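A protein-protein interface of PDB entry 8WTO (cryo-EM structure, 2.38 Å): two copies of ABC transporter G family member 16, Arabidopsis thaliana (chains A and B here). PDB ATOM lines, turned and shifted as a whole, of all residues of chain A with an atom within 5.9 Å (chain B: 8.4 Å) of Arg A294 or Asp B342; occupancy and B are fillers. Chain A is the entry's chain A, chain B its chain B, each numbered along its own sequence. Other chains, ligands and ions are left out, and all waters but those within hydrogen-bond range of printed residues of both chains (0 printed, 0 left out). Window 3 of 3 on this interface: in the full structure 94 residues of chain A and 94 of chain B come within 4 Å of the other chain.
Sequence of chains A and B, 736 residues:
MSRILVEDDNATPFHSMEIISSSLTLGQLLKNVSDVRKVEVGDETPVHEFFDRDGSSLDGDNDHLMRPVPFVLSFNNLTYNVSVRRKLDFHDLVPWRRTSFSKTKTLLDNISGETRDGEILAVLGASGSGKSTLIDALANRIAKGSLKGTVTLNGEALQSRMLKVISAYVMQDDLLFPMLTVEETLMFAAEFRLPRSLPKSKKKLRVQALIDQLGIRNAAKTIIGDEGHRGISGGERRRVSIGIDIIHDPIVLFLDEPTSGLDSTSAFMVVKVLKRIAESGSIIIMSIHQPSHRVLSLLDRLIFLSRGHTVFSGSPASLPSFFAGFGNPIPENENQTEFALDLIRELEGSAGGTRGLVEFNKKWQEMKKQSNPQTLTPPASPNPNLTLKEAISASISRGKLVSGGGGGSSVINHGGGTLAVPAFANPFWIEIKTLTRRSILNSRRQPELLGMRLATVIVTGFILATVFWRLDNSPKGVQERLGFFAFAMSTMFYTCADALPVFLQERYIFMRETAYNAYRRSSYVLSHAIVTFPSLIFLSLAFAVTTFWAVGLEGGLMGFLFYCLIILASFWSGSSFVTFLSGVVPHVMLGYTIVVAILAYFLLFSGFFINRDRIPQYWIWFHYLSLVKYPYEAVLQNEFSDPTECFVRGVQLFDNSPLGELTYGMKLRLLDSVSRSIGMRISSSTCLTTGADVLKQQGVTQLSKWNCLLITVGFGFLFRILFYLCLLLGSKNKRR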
ATOM      1  N   SER A 264       8.849  16.419  13.694  1.00  0.00           N
ATOM      2  CA  SER A 264       7.833  17.068  14.512  1.00  0.00           C
ATOM      3  C   SER A 264       7.637  16.385  15.861  1.00  0.00           C
ATOM      4  O   SER A 264       7.266  17.049  16.832  1.00  0.00           O
ATOM      5  CB  SER A 264       6.518  17.113  13.746  1.00  0.00           C
ATOM      6  OG  SER A 264       6.100  15.812  13.382  1.00  0.00           O
ATOM      7  N   THR A 265       7.898  15.085  15.956  1.00  0.00           N
ATOM      8  CA  THR A 265       7.733  14.409  17.236  1.00  0.00           C
ATOM      9  C   THR A 265       8.977  14.483  18.109  1.00  0.00           C
ATOM     10  O   THR A 265       8.859  14.420  19.336  1.00  0.00           O
ATOM     11  CB  THR A 265       7.302  12.944  17.032  1.00  0.00           C
ATOM     12  OG1 THR A 265       7.135  12.303  18.301  1.00  0.00           O
ATOM     13  CG2 THR A 265       8.287  12.165  16.215  1.00  0.00           C
ATOM     14  N   PHE A 268       8.994  18.129  19.516  1.00  0.00           N
ATOM     15  CA  PHE A 268       8.111  18.186  20.673  1.00  0.00           C
ATOM     16  C   PHE A 268       8.763  17.588  21.911  1.00  0.00           C
ATOM     17  O   PHE A 268       8.526  18.065  23.023  1.00  0.00           O
ATOM     18  CB  PHE A 268       6.809  17.459  20.348  1.00  0.00           C
ATOM     19  CG  PHE A 268       5.710  17.705  21.329  1.00  0.00           C
ATOM     20  CD1 PHE A 268       5.394  18.989  21.735  1.00  0.00           C
ATOM     21  CD2 PHE A 268       4.971  16.648  21.831  1.00  0.00           C
ATOM     22  CE1 PHE A 268       4.371  19.211  22.635  1.00  0.00           C
ATOM     23  CE2 PHE A 268       3.945  16.865  22.728  1.00  0.00           C
ATOM     24  CZ  PHE A 268       3.648  18.147  23.133  1.00  0.00           C
ATOM     25  N   SER A 292       4.942  24.003  15.641  1.00  0.00           N
ATOM     26  CA  SER A 292       3.595  23.488  15.517  1.00  0.00           C
ATOM     27  C   SER A 292       2.739  24.025  16.657  1.00  0.00           C
ATOM     28  O   SER A 292       3.221  24.690  17.577  1.00  0.00           O
ATOM     29  CB  SER A 292       3.617  21.967  15.507  1.00  0.00           C
ATOM     30  OG  SER A 292       4.081  21.465  16.742  1.00  0.00           O
ATOM     31  N   HIS A 293       1.443  23.725  16.603  1.00  0.00           N
ATOM     32  CA  HIS A 293       0.541  24.137  17.667  1.00  0.00           C
ATOM     33  C   HIS A 293       0.798  23.383  18.967  1.00  0.00           C
ATOM     34  O   HIS A 293       0.432  23.878  20.036  1.00  0.00           O
ATOM     35  CB  HIS A 293      -0.905  23.952  17.216  1.00  0.00           C
ATOM     36  CG  HIS A 293      -1.894  24.713  18.038  1.00  0.00           C
ATOM     37  ND1 HIS A 293      -2.529  24.166  19.132  1.00  0.00           N
ATOM     38  CD2 HIS A 293      -2.360  25.979  17.926  1.00  0.00           C
ATOM     39  CE1 HIS A 293      -3.343  25.062  19.659  1.00  0.00           C
ATOM     40  NE2 HIS A 293      -3.259  26.171  18.945  1.00  0.00           N
ATOM     41  N   ARG A 294       1.412  22.200  18.895  1.00  0.00           N
ATOM     42  CA  ARG A 294       1.876  21.523  20.103  1.00  0.00           C
ATOM     43  C   ARG A 294       3.023  22.278  20.758  1.00  0.00           C
ATOM     44  O   ARG A 294       3.043  22.445  21.982  1.00  0.00           O
ATOM     45  CB  ARG A 294       2.324  20.103  19.772  1.00  0.00           C
ATOM     46  CG  ARG A 294       1.219  19.100  19.630  1.00  0.00           C
ATOM     47  CD  ARG A 294       1.785  17.693  19.658  1.00  0.00           C
ATOM     48  NE  ARG A 294       2.872  17.517  18.702  1.00  0.00           N
ATOM     49  CZ  ARG A 294       3.378  16.337  18.365  1.00  0.00           C
ATOM     50  NH1 ARG A 294       2.891  15.233  18.906  1.00  0.00           N
ATOM     51  NH2 ARG A 294       4.368  16.259  17.490  1.00  0.00           N
ATOM     52  N   VAL A 295       3.998  22.720  19.962  1.00  0.00           N
ATOM     53  CA  VAL A 295       5.176  23.384  20.510  1.00  0.00           C
ATOM     54  C   VAL A 295       4.827  24.788  20.984  1.00  0.00           C
ATOM     55  O   VAL A 295       5.240  25.210  22.071  1.00  0.00           O
ATOM     56  CB  VAL A 295       6.306  23.383  19.463  1.00  0.00           C
ATOM     57  CG1 VAL A 295       7.422  24.324  19.855  1.00  0.00           C
ATOM     58  CG2 VAL A 295       6.842  21.980  19.286  1.00  0.00           C
ATOM     59  N   LEU A 296       4.012  25.508  20.206  1.00  0.00           N
ATOM     60  CA  LEU A 296       3.622  26.877  20.524  1.00  0.00           C
ATOM     61  C   LEU A 296       2.804  26.983  21.803  1.00  0.00           C
ATOM     62  O   LEU A 296       2.818  28.038  22.445  1.00  0.00           O
ATOM     63  CB  LEU A 296       2.833  27.472  19.361  1.00  0.00           C
ATOM     64  CG  LEU A 296       2.788  28.992  19.232  1.00  0.00           C
ATOM     65  CD1 LEU A 296       4.083  29.520  18.659  1.00  0.00           C
ATOM     66  CD2 LEU A 296       1.612  29.410  18.376  1.00  0.00           C
ATOM     67  N   SER A 297       2.109  25.916  22.198  1.00  0.00           N
ATOM     68  CA  SER A 297       1.404  25.925  23.471  1.00  0.00           C
ATOM     69  C   SER A 297       2.354  25.782  24.651  1.00  0.00           C
ATOM     70  O   SER A 297       1.987  26.135  25.774  1.00  0.00           O
ATOM     71  CB  SER A 297       0.362  24.809  23.503  1.00  0.00           C
ATOM     72  OG  SER A 297       0.974  23.531  23.527  1.00  0.00           O
ATOM     73  N   LEU A 298       3.564  25.273  24.423  1.00  0.00           N
ATOM     74  CA  LEU A 298       4.557  25.166  25.481  1.00  0.00           C
ATOM     75  C   LEU A 298       5.374  26.437  25.658  1.00  0.00           C
ATOM     76  O   LEU A 298       6.102  26.546  26.647  1.00  0.00           O
ATOM     77  CB  LEU A 298       5.504  23.999  25.206  1.00  0.00           C
ATOM     78  CG  LEU A 298       4.928  22.591  25.145  1.00  0.00           C
ATOM     79  CD1 LEU A 298       6.022  21.621  24.764  1.00  0.00           C
ATOM     80  CD2 LEU A 298       4.314  22.198  26.472  1.00  0.00           C
ATOM     81  N   ALA B 126      11.526  10.179  10.970  1.00  0.00           N
ATOM     82  CA  ALA B 126      12.174  10.735  12.140  1.00  0.00           C
ATOM     83  C   ALA B 126      13.656  10.976  11.869  1.00  0.00           C
ATOM     84  O   ALA B 126      14.226  10.506  10.884  1.00  0.00           O
ATOM     85  CB  ALA B 126      11.992   9.811  13.340  1.00  0.00           C
ATOM     86  N   GLN B 290       9.271  19.178   9.030  1.00  0.00           N
ATOM     87  CA  GLN B 290       8.007  19.658   9.584  1.00  0.00           C
ATOM     88  C   GLN B 290       7.241  20.447   8.531  1.00  0.00           C
ATOM     89  O   GLN B 290       7.089  21.669   8.661  1.00  0.00           O
ATOM     90  CB  GLN B 290       8.241  20.507  10.830  1.00  0.00           C
ATOM     91  CG  GLN B 290       8.994  19.798  11.942  1.00  0.00           C
ATOM     92  CD  GLN B 290       9.394  20.729  13.063  1.00  0.00           C
ATOM     93  OE1 GLN B 290       8.600  21.552  13.510  1.00  0.00           O
ATOM     94  NE2 GLN B 290      10.628  20.604  13.523  1.00  0.00           N
ATOM     95  N   PHE B 304       7.593   7.625   3.676  1.00  0.00           N
ATOM     96  CA  PHE B 304       7.867   7.719   5.102  1.00  0.00           C
ATOM     97  C   PHE B 304       8.852   6.627   5.484  1.00  0.00           C
ATOM     98  O   PHE B 304       8.649   5.459   5.147  1.00  0.00           O
ATOM     99  CB  PHE B 304       6.584   7.572   5.920  1.00  0.00           C
ATOM    100  CG  PHE B 304       5.763   8.825   6.016  1.00  0.00           C
ATOM    101  CD1 PHE B 304       5.444   9.357   7.247  1.00  0.00           C
ATOM    102  CD2 PHE B 304       5.291   9.457   4.882  1.00  0.00           C
ATOM    103  CE1 PHE B 304       4.677  10.499   7.338  1.00  0.00           C
ATOM    104  CE2 PHE B 304       4.530  10.598   4.971  1.00  0.00           C
ATOM    105  CZ  PHE B 304       4.224  11.118   6.198  1.00  0.00           C
ATOM    106  N   PHE B 323      -4.019   5.060   7.147  1.00  0.00           N
ATOM    107  CA  PHE B 323      -3.917   4.737   8.565  1.00  0.00           C
ATOM    108  C   PHE B 323      -5.258   4.303   9.139  1.00  0.00           C
ATOM    109  O   PHE B 323      -5.303   3.651  10.187  1.00  0.00           O
ATOM    110  CB  PHE B 323      -3.343   5.928   9.331  1.00  0.00           C
ATOM    111  CG  PHE B 323      -1.849   6.011   9.263  1.00  0.00           C
ATOM    112  CD1 PHE B 323      -1.065   5.163  10.021  1.00  0.00           C
ATOM    113  CD2 PHE B 323      -1.227   6.912   8.415  1.00  0.00           C
ATOM    114  CE1 PHE B 323       0.311   5.220   9.949  1.00  0.00           C
ATOM    115  CE2 PHE B 323       0.152   6.975   8.340  1.00  0.00           C
ATOM    116  CZ  PHE B 323       0.921   6.128   9.108  1.00  0.00           C
ATOM    117  N   GLU B 334      -6.293  17.233  13.419  1.00  0.00           N
ATOM    118  CA  GLU B 334      -4.870  17.106  13.696  1.00  0.00           C
ATOM    119  C   GLU B 334      -4.054  17.120  12.411  1.00  0.00           C
ATOM    120  O   GLU B 334      -4.566  16.863  11.319  1.00  0.00           O
ATOM    121  CB  GLU B 334      -4.556  15.826  14.476  1.00  0.00           C
ATOM    122  CG  GLU B 334      -4.984  15.846  15.931  1.00  0.00           C
ATOM    123  CD  GLU B 334      -4.536  14.608  16.682  1.00  0.00           C
ATOM    124  OE1 GLU B 334      -4.024  13.672  16.036  1.00  0.00           O
ATOM    125  OE2 GLU B 334      -4.680  14.577  17.923  1.00  0.00           O
ATOM    126  N   ASN B 335      -2.767  17.433  12.561  1.00  0.00           N
ATOM    127  CA  ASN B 335      -1.840  17.388  11.440  1.00  0.00           C
ATOM    128  C   ASN B 335      -1.566  15.938  11.065  1.00  0.00           C
ATOM    129  O   ASN B 335      -1.299  15.103  11.932  1.00  0.00           O
ATOM    130  CB  ASN B 335      -0.544  18.106  11.802  1.00  0.00           C
ATOM    131  CG  ASN B 335       0.287  18.463  10.587  1.00  0.00           C
ATOM    132  OD1 ASN B 335      -0.004  19.433   9.889  1.00  0.00           O
ATOM    133  ND2 ASN B 335       1.323  17.678  10.324  1.00  0.00           N
ATOM    134  N   GLN B 336      -1.638  15.638   9.768  1.00  0.00           N
ATOM    135  CA  GLN B 336      -1.582  14.249   9.331  1.00  0.00           C
ATOM    136  C   GLN B 336      -0.164  13.694   9.365  1.00  0.00           C
ATOM    137  O   GLN B 336       0.032  12.518   9.688  1.00  0.00           O
ATOM    138  CB  GLN B 336      -2.185  14.120   7.934  1.00  0.00           C
ATOM    139  CG  GLN B 336      -3.692  14.288   7.921  1.00  0.00           C
ATOM    140  CD  GLN B 336      -4.262  14.392   6.523  1.00  0.00           C
ATOM    141  OE1 GLN B 336      -3.531  14.601   5.556  1.00  0.00           O
ATOM    142  NE2 GLN B 336      -5.575  14.244   6.408  1.00  0.00           N
ATOM    143  N   THR B 337       0.839  14.512   9.046  1.00  0.00           N
ATOM    144  CA  THR B 337       2.209  14.030   9.156  1.00  0.00           C
ATOM    145  C   THR B 337       2.685  14.003  10.600  1.00  0.00           C
ATOM    146  O   THR B 337       3.511  13.158  10.953  1.00  0.00           O
ATOM    147  CB  THR B 337       3.156  14.876   8.299  1.00  0.00           C
ATOM    148  OG1 THR B 337       2.935  16.267   8.550  1.00  0.00           O
ATOM    149  CG2 THR B 337       2.930  14.590   6.831  1.00  0.00           C
ATOM    150  N   GLU B 338       2.170  14.896  11.449  1.00  0.00           N
ATOM    151  CA  GLU B 338       2.494  14.839  12.871  1.00  0.00           C
ATOM    152  C   GLU B 338       1.902  13.601  13.527  1.00  0.00           C
ATOM    153  O   GLU B 338       2.546  12.981  14.379  1.00  0.00           O
ATOM    154  CB  GLU B 338       1.992  16.089  13.585  1.00  0.00           C
ATOM    155  CG  GLU B 338       2.825  17.316  13.352  1.00  0.00           C
ATOM    156  CD  GLU B 338       2.856  18.220  14.558  1.00  0.00           C
ATOM    157  OE1 GLU B 338       1.826  18.329  15.255  1.00  0.00           O
ATOM    158  OE2 GLU B 338       3.918  18.811  14.817  1.00  0.00           O
ATOM    159  N   PHE B 339       0.672  13.238  13.152  1.00  0.00           N
ATOM    160  CA  PHE B 339       0.057  12.022  13.672  1.00  0.00           C
ATOM    161  C   PHE B 339       0.774  10.779  13.173  1.00  0.00           C
ATOM    162  O   PHE B 339       0.848   9.780  13.894  1.00  0.00           O
ATOM    163  CB  PHE B 339      -1.423  11.973  13.278  1.00  0.00           C
ATOM    164  CG  PHE B 339      -2.169  10.786  13.833  1.00  0.00           C
ATOM    165  CD1 PHE B 339      -2.357   9.639  13.071  1.00  0.00           C
ATOM    166  CD2 PHE B 339      -2.696  10.826  15.113  1.00  0.00           C
ATOM    167  CE1 PHE B 339      -3.042   8.556  13.580  1.00  0.00           C
ATOM    168  CE2 PHE B 339      -3.385   9.745  15.626  1.00  0.00           C
ATOM    169  CZ  PHE B 339      -3.556   8.609  14.858  1.00  0.00           C
ATOM    170  N   ALA B 340       1.288  10.821  11.944  1.00  0.00           N
ATOM    171  CA  ALA B 340       1.930   9.654  11.356  1.00  0.00           C
ATOM    172  C   ALA B 340       3.247   9.343  12.050  1.00  0.00           C
ATOM    173  O   ALA B 340       3.482   8.205  12.466  1.00  0.00           O
ATOM    174  CB  ALA B 340       2.137   9.875   9.861  1.00  0.00           C
ATOM    175  N   LEU B 341       4.107  10.351  12.216  1.00  0.00           N
ATOM    176  CA  LEU B 341       5.375  10.139  12.902  1.00  0.00           C
ATOM    177  C   LEU B 341       5.203   9.920  14.399  1.00  0.00           C
ATOM    178  O   LEU B 341       6.099   9.353  15.030  1.00  0.00           O
ATOM    179  CB  LEU B 341       6.330  11.310  12.662  1.00  0.00           C
ATOM    180  CG  LEU B 341       7.168  11.331  11.379  1.00  0.00           C
ATOM    181  CD1 LEU B 341       6.391  11.793  10.178  1.00  0.00           C
ATOM    182  CD2 LEU B 341       8.384  12.189  11.562  1.00  0.00           C
ATOM    183  N   ASP B 342       4.085  10.360  14.982  1.00  0.00           N
ATOM    184  CA  ASP B 342       3.786  10.003  16.365  1.00  0.00           C
ATOM    185  C   ASP B 342       3.501   8.514  16.498  1.00  0.00           C
ATOM    186  O   ASP B 342       4.018   7.857  17.407  1.00  0.00           O
ATOM    187  CB  ASP B 342       2.595  10.810  16.873  1.00  0.00           C
ATOM    188  CG  ASP B 342       2.987  12.174  17.383  1.00  0.00           C
ATOM    189  OD1 ASP B 342       4.129  12.328  17.853  1.00  0.00           O
ATOM    190  OD2 ASP B 342       2.151  13.097  17.316  1.00  0.00           O
ATOM    191  N   LEU B 343       2.683   7.968  15.593  1.00  0.00           N
ATOM    192  CA  LEU B 343       2.348   6.549  15.631  1.00  0.00           C
ATOM    193  C   LEU B 343       3.545   5.682  15.273  1.00  0.00           C
ATOM    194  O   LEU B 343       3.724   4.600  15.840  1.00  0.00           O
ATOM    195  CB  LEU B 343       1.185   6.263  14.683  1.00  0.00           C
ATOM    196  CG  LEU B 343       0.632   4.841  14.726  1.00  0.00           C
ATOM    197  CD1 LEU B 343      -0.138   4.628  16.014  1.00  0.00           C
ATOM    198  CD2 LEU B 343      -0.232   4.553  13.519  1.00  0.00           C
ATOM    199  N   ILE B 344       4.375   6.149  14.340  1.00  0.00           N
ATOM    200  CA  ILE B 344       5.536   5.386  13.893  1.00  0.00           C
ATOM    201  C   ILE B 344       6.575   5.282  15.006  1.00  0.00           C
ATOM    202  O   ILE B 344       7.152   4.211  15.234  1.00  0.00           O
ATOM    203  CB  ILE B 344       6.101   6.031  12.611  1.00  0.00           C
ATOM    204  CG1 ILE B 344       5.257   5.631  11.401  1.00  0.00           C
ATOM    205  CG2 ILE B 344       7.546   5.665  12.374  1.00  0.00           C
ATOM    206  CD1 ILE B 344       5.331   6.615  10.260  1.00  0.00           C
ATOM    207  N   ARG B 345       6.800   6.375  15.741  1.00  0.00           N
ATOM    208  CA  ARG B 345       7.739   6.351  16.859  1.00  0.00           C
ATOM    209  C   ARG B 345       7.217   5.492  18.010  1.00  0.00           C
ATOM    210  O   ARG B 345       7.989   4.779  18.662  1.00  0.00           O
ATOM    211  CB  ARG B 345       8.034   7.786  17.315  1.00  0.00           C
ATOM    212  CG  ARG B 345       8.566   7.925  18.734  1.00  0.00           C
ATOM    213  CD  ARG B 345       9.652   8.975  18.861  1.00  0.00           C
ATOM    214  NE  ARG B 345      10.184   9.018  20.220  1.00  0.00           N
ATOM    215  CZ  ARG B 345      11.327   8.455  20.600  1.00  0.00           C
ATOM    216  NH1 ARG B 345      12.078   7.813  19.718  1.00  0.00           N
ATOM    217  NH2 ARG B 345      11.723   8.540  21.862  1.00  0.00           N
ATOM    218  N   GLU B 346       5.902   5.525  18.249  1.00  0.00           N
ATOM    219  CA  GLU B 346       5.289   4.635  19.232  1.00  0.00           C
ATOM    220  C   GLU B 346       5.412   3.173  18.812  1.00  0.00           C
ATOM    221  O   GLU B 346       5.634   2.296  19.656  1.00  0.00           O
ATOM    222  CB  GLU B 346       3.822   5.020  19.428  1.00  0.00           C
ATOM    223  CG  GLU B 346       3.056   4.156  20.413  1.00  0.00           C
ATOM    224  CD  GLU B 346       1.552   4.320  20.287  1.00  0.00           C
ATOM    225  OE1 GLU B 346       0.815   3.631  21.021  1.00  0.00           O
ATOM    226  OE2 GLU B 346       1.110   5.141  19.456  1.00  0.00           O
ATOM    227  N   LEU B 347       5.295   2.895  17.512  1.00  0.00           N
ATOM    228  CA  LEU B 347       5.487   1.535  17.022  1.00  0.00           C
ATOM    229  C   LEU B 347       6.941   1.097  17.131  1.00  0.00           C
ATOM    230  O   LEU B 347       7.207  -0.094  17.306  1.00  0.00           O
ATOM    231  CB  LEU B 347       5.013   1.418  15.574  1.00  0.00           C
ATOM    232  CG  LEU B 347       3.512   1.323  15.313  1.00  0.00           C
ATOM    233  CD1 LEU B 347       3.259   0.980  13.858  1.00  0.00           C
ATOM    234  CD2 LEU B 347       2.857   0.309  16.232  1.00  0.00           C
ATOM    235  N   GLU B 348       7.885   2.037  17.036  1.00  0.00           N
ATOM    236  CA  GLU B 348       9.298   1.711  17.205  1.00  0.00           C
ATOM    237  C   GLU B 348       9.611   1.247  18.622  1.00  0.00           C
ATOM    238  O   GLU B 348      10.494   0.406  18.814  1.00  0.00           O
ATOM    239  CB  GLU B 348      10.163   2.921  16.861  1.00  0.00           C
ATOM    240  CG  GLU B 348      10.437   3.113  15.387  1.00  0.00           C
ATOM    241  CD  GLU B 348      11.036   4.473  15.093  1.00  0.00           C
ATOM    242  OE1 GLU B 348      10.353   5.306  14.462  1.00  0.00           O
ATOM    243  OE2 GLU B 348      12.190   4.712  15.505  1.00  0.00           O
ATOM    244  N   GLY B 349       8.910   1.779  19.615  1.00  0.00           N
ATOM    245  CA  GLY B 349       9.092   1.372  20.989  1.00  0.00           C
ATOM    246  C   GLY B 349       8.240   0.211  21.430  1.00  0.00           C
ATOM    247  O   GLY B 349       8.377  -0.247  22.568  1.00  0.00           O
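OD2 of Asp B342 is in salt-bridge range of NH1 of Arg A294 (2.8 Å).
The side-chain hydroxyl (OG1) of Thr A265 lies within hydrogen-bond range of the side-chain carboxylate (OD1) of Asp B342 (3.0 Å).
The side-chain hydroxyl (OG) of Ser A292 lies close to the side-chain carboxylate (OE2) of Glu B338.
The guanidinium group of Arg A294 is in salt-bridge range of the side-chain carboxylate of Glu B338, at 3.7 Å.
No position is printed for both chains.
Of the 7 pairs that touch across the chains among the printed residues, none has its exchanged pair printed and touching as well.
The side-chain amide nitrogen of Asn B335 lies close to the backbone NH of Glu B338 (3.1 Å).
O of Ser A264 is in hydrogen-bond range of NH2 of Arg A294 (3.1 Å).
The side-chain hydroxyl (OG) of Ser A292 sits at hydrogen-bond distance from the backbone NH (N) of Val A295, at 3.5 Å.
The backbone carbonyl oxygen of Arg A294 sits at hydrogen-bond distance from the side-chain hydroxyl of Ser A297, at 2.8 Å.
Among the printed residues, merely in contact across the chains: Ser A264 with Glu B338, Thr A265 with Leu B341 and Ser A264 with Gln B290.
Printed residues of chain B that touch a printed residue of chain A: Gln B290, Glu B338, Leu B341 and Asp B342.
Along chain B the printed residues that touch a printed residue of chain A span positions 290 to 342.
Of the 10 printed residues of chain A, 4 touch a printed residue of chain B.
Among the printed residues, 7 pairs touch across the chains.
Among the printed residues, Asp or Glu carboxylates within 4 Å of a Lys or Arg side-chain nitrogen of the other chain: Arg A294 with Glu B338 (3.7 Å) and Arg A294 with Asp B342 (2.8 Å).
Arg A294 touches just these residues of chain B: Glu B338 (3.7 Å) and Asp B342 (2.8 Å).
Asp B342 touches just these residues of chain A: Thr A265 and Arg A294.
Of the printed residues of chain A, Gln B290 touches Ser A264 (3.8 Å).
Printed residues of chain B within 4 Å of Ser A292: Glu B338.
Of the printed residues of chain A, Leu B341 touches Thr A265.
Of the printed residues of chain B, Ser A264 touches Gln B290 and Glu B338.
The nearest residue of chain B that does not touch Arg A294 is Phe B339 (6.5 Å).
The nearest residue of chain A that does not touch Asp B342 is Ser A264 (5.7 Å).
The nearest printed residue of chain A that does not touch Glu B338 is Thr A265 (5.4 Å).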
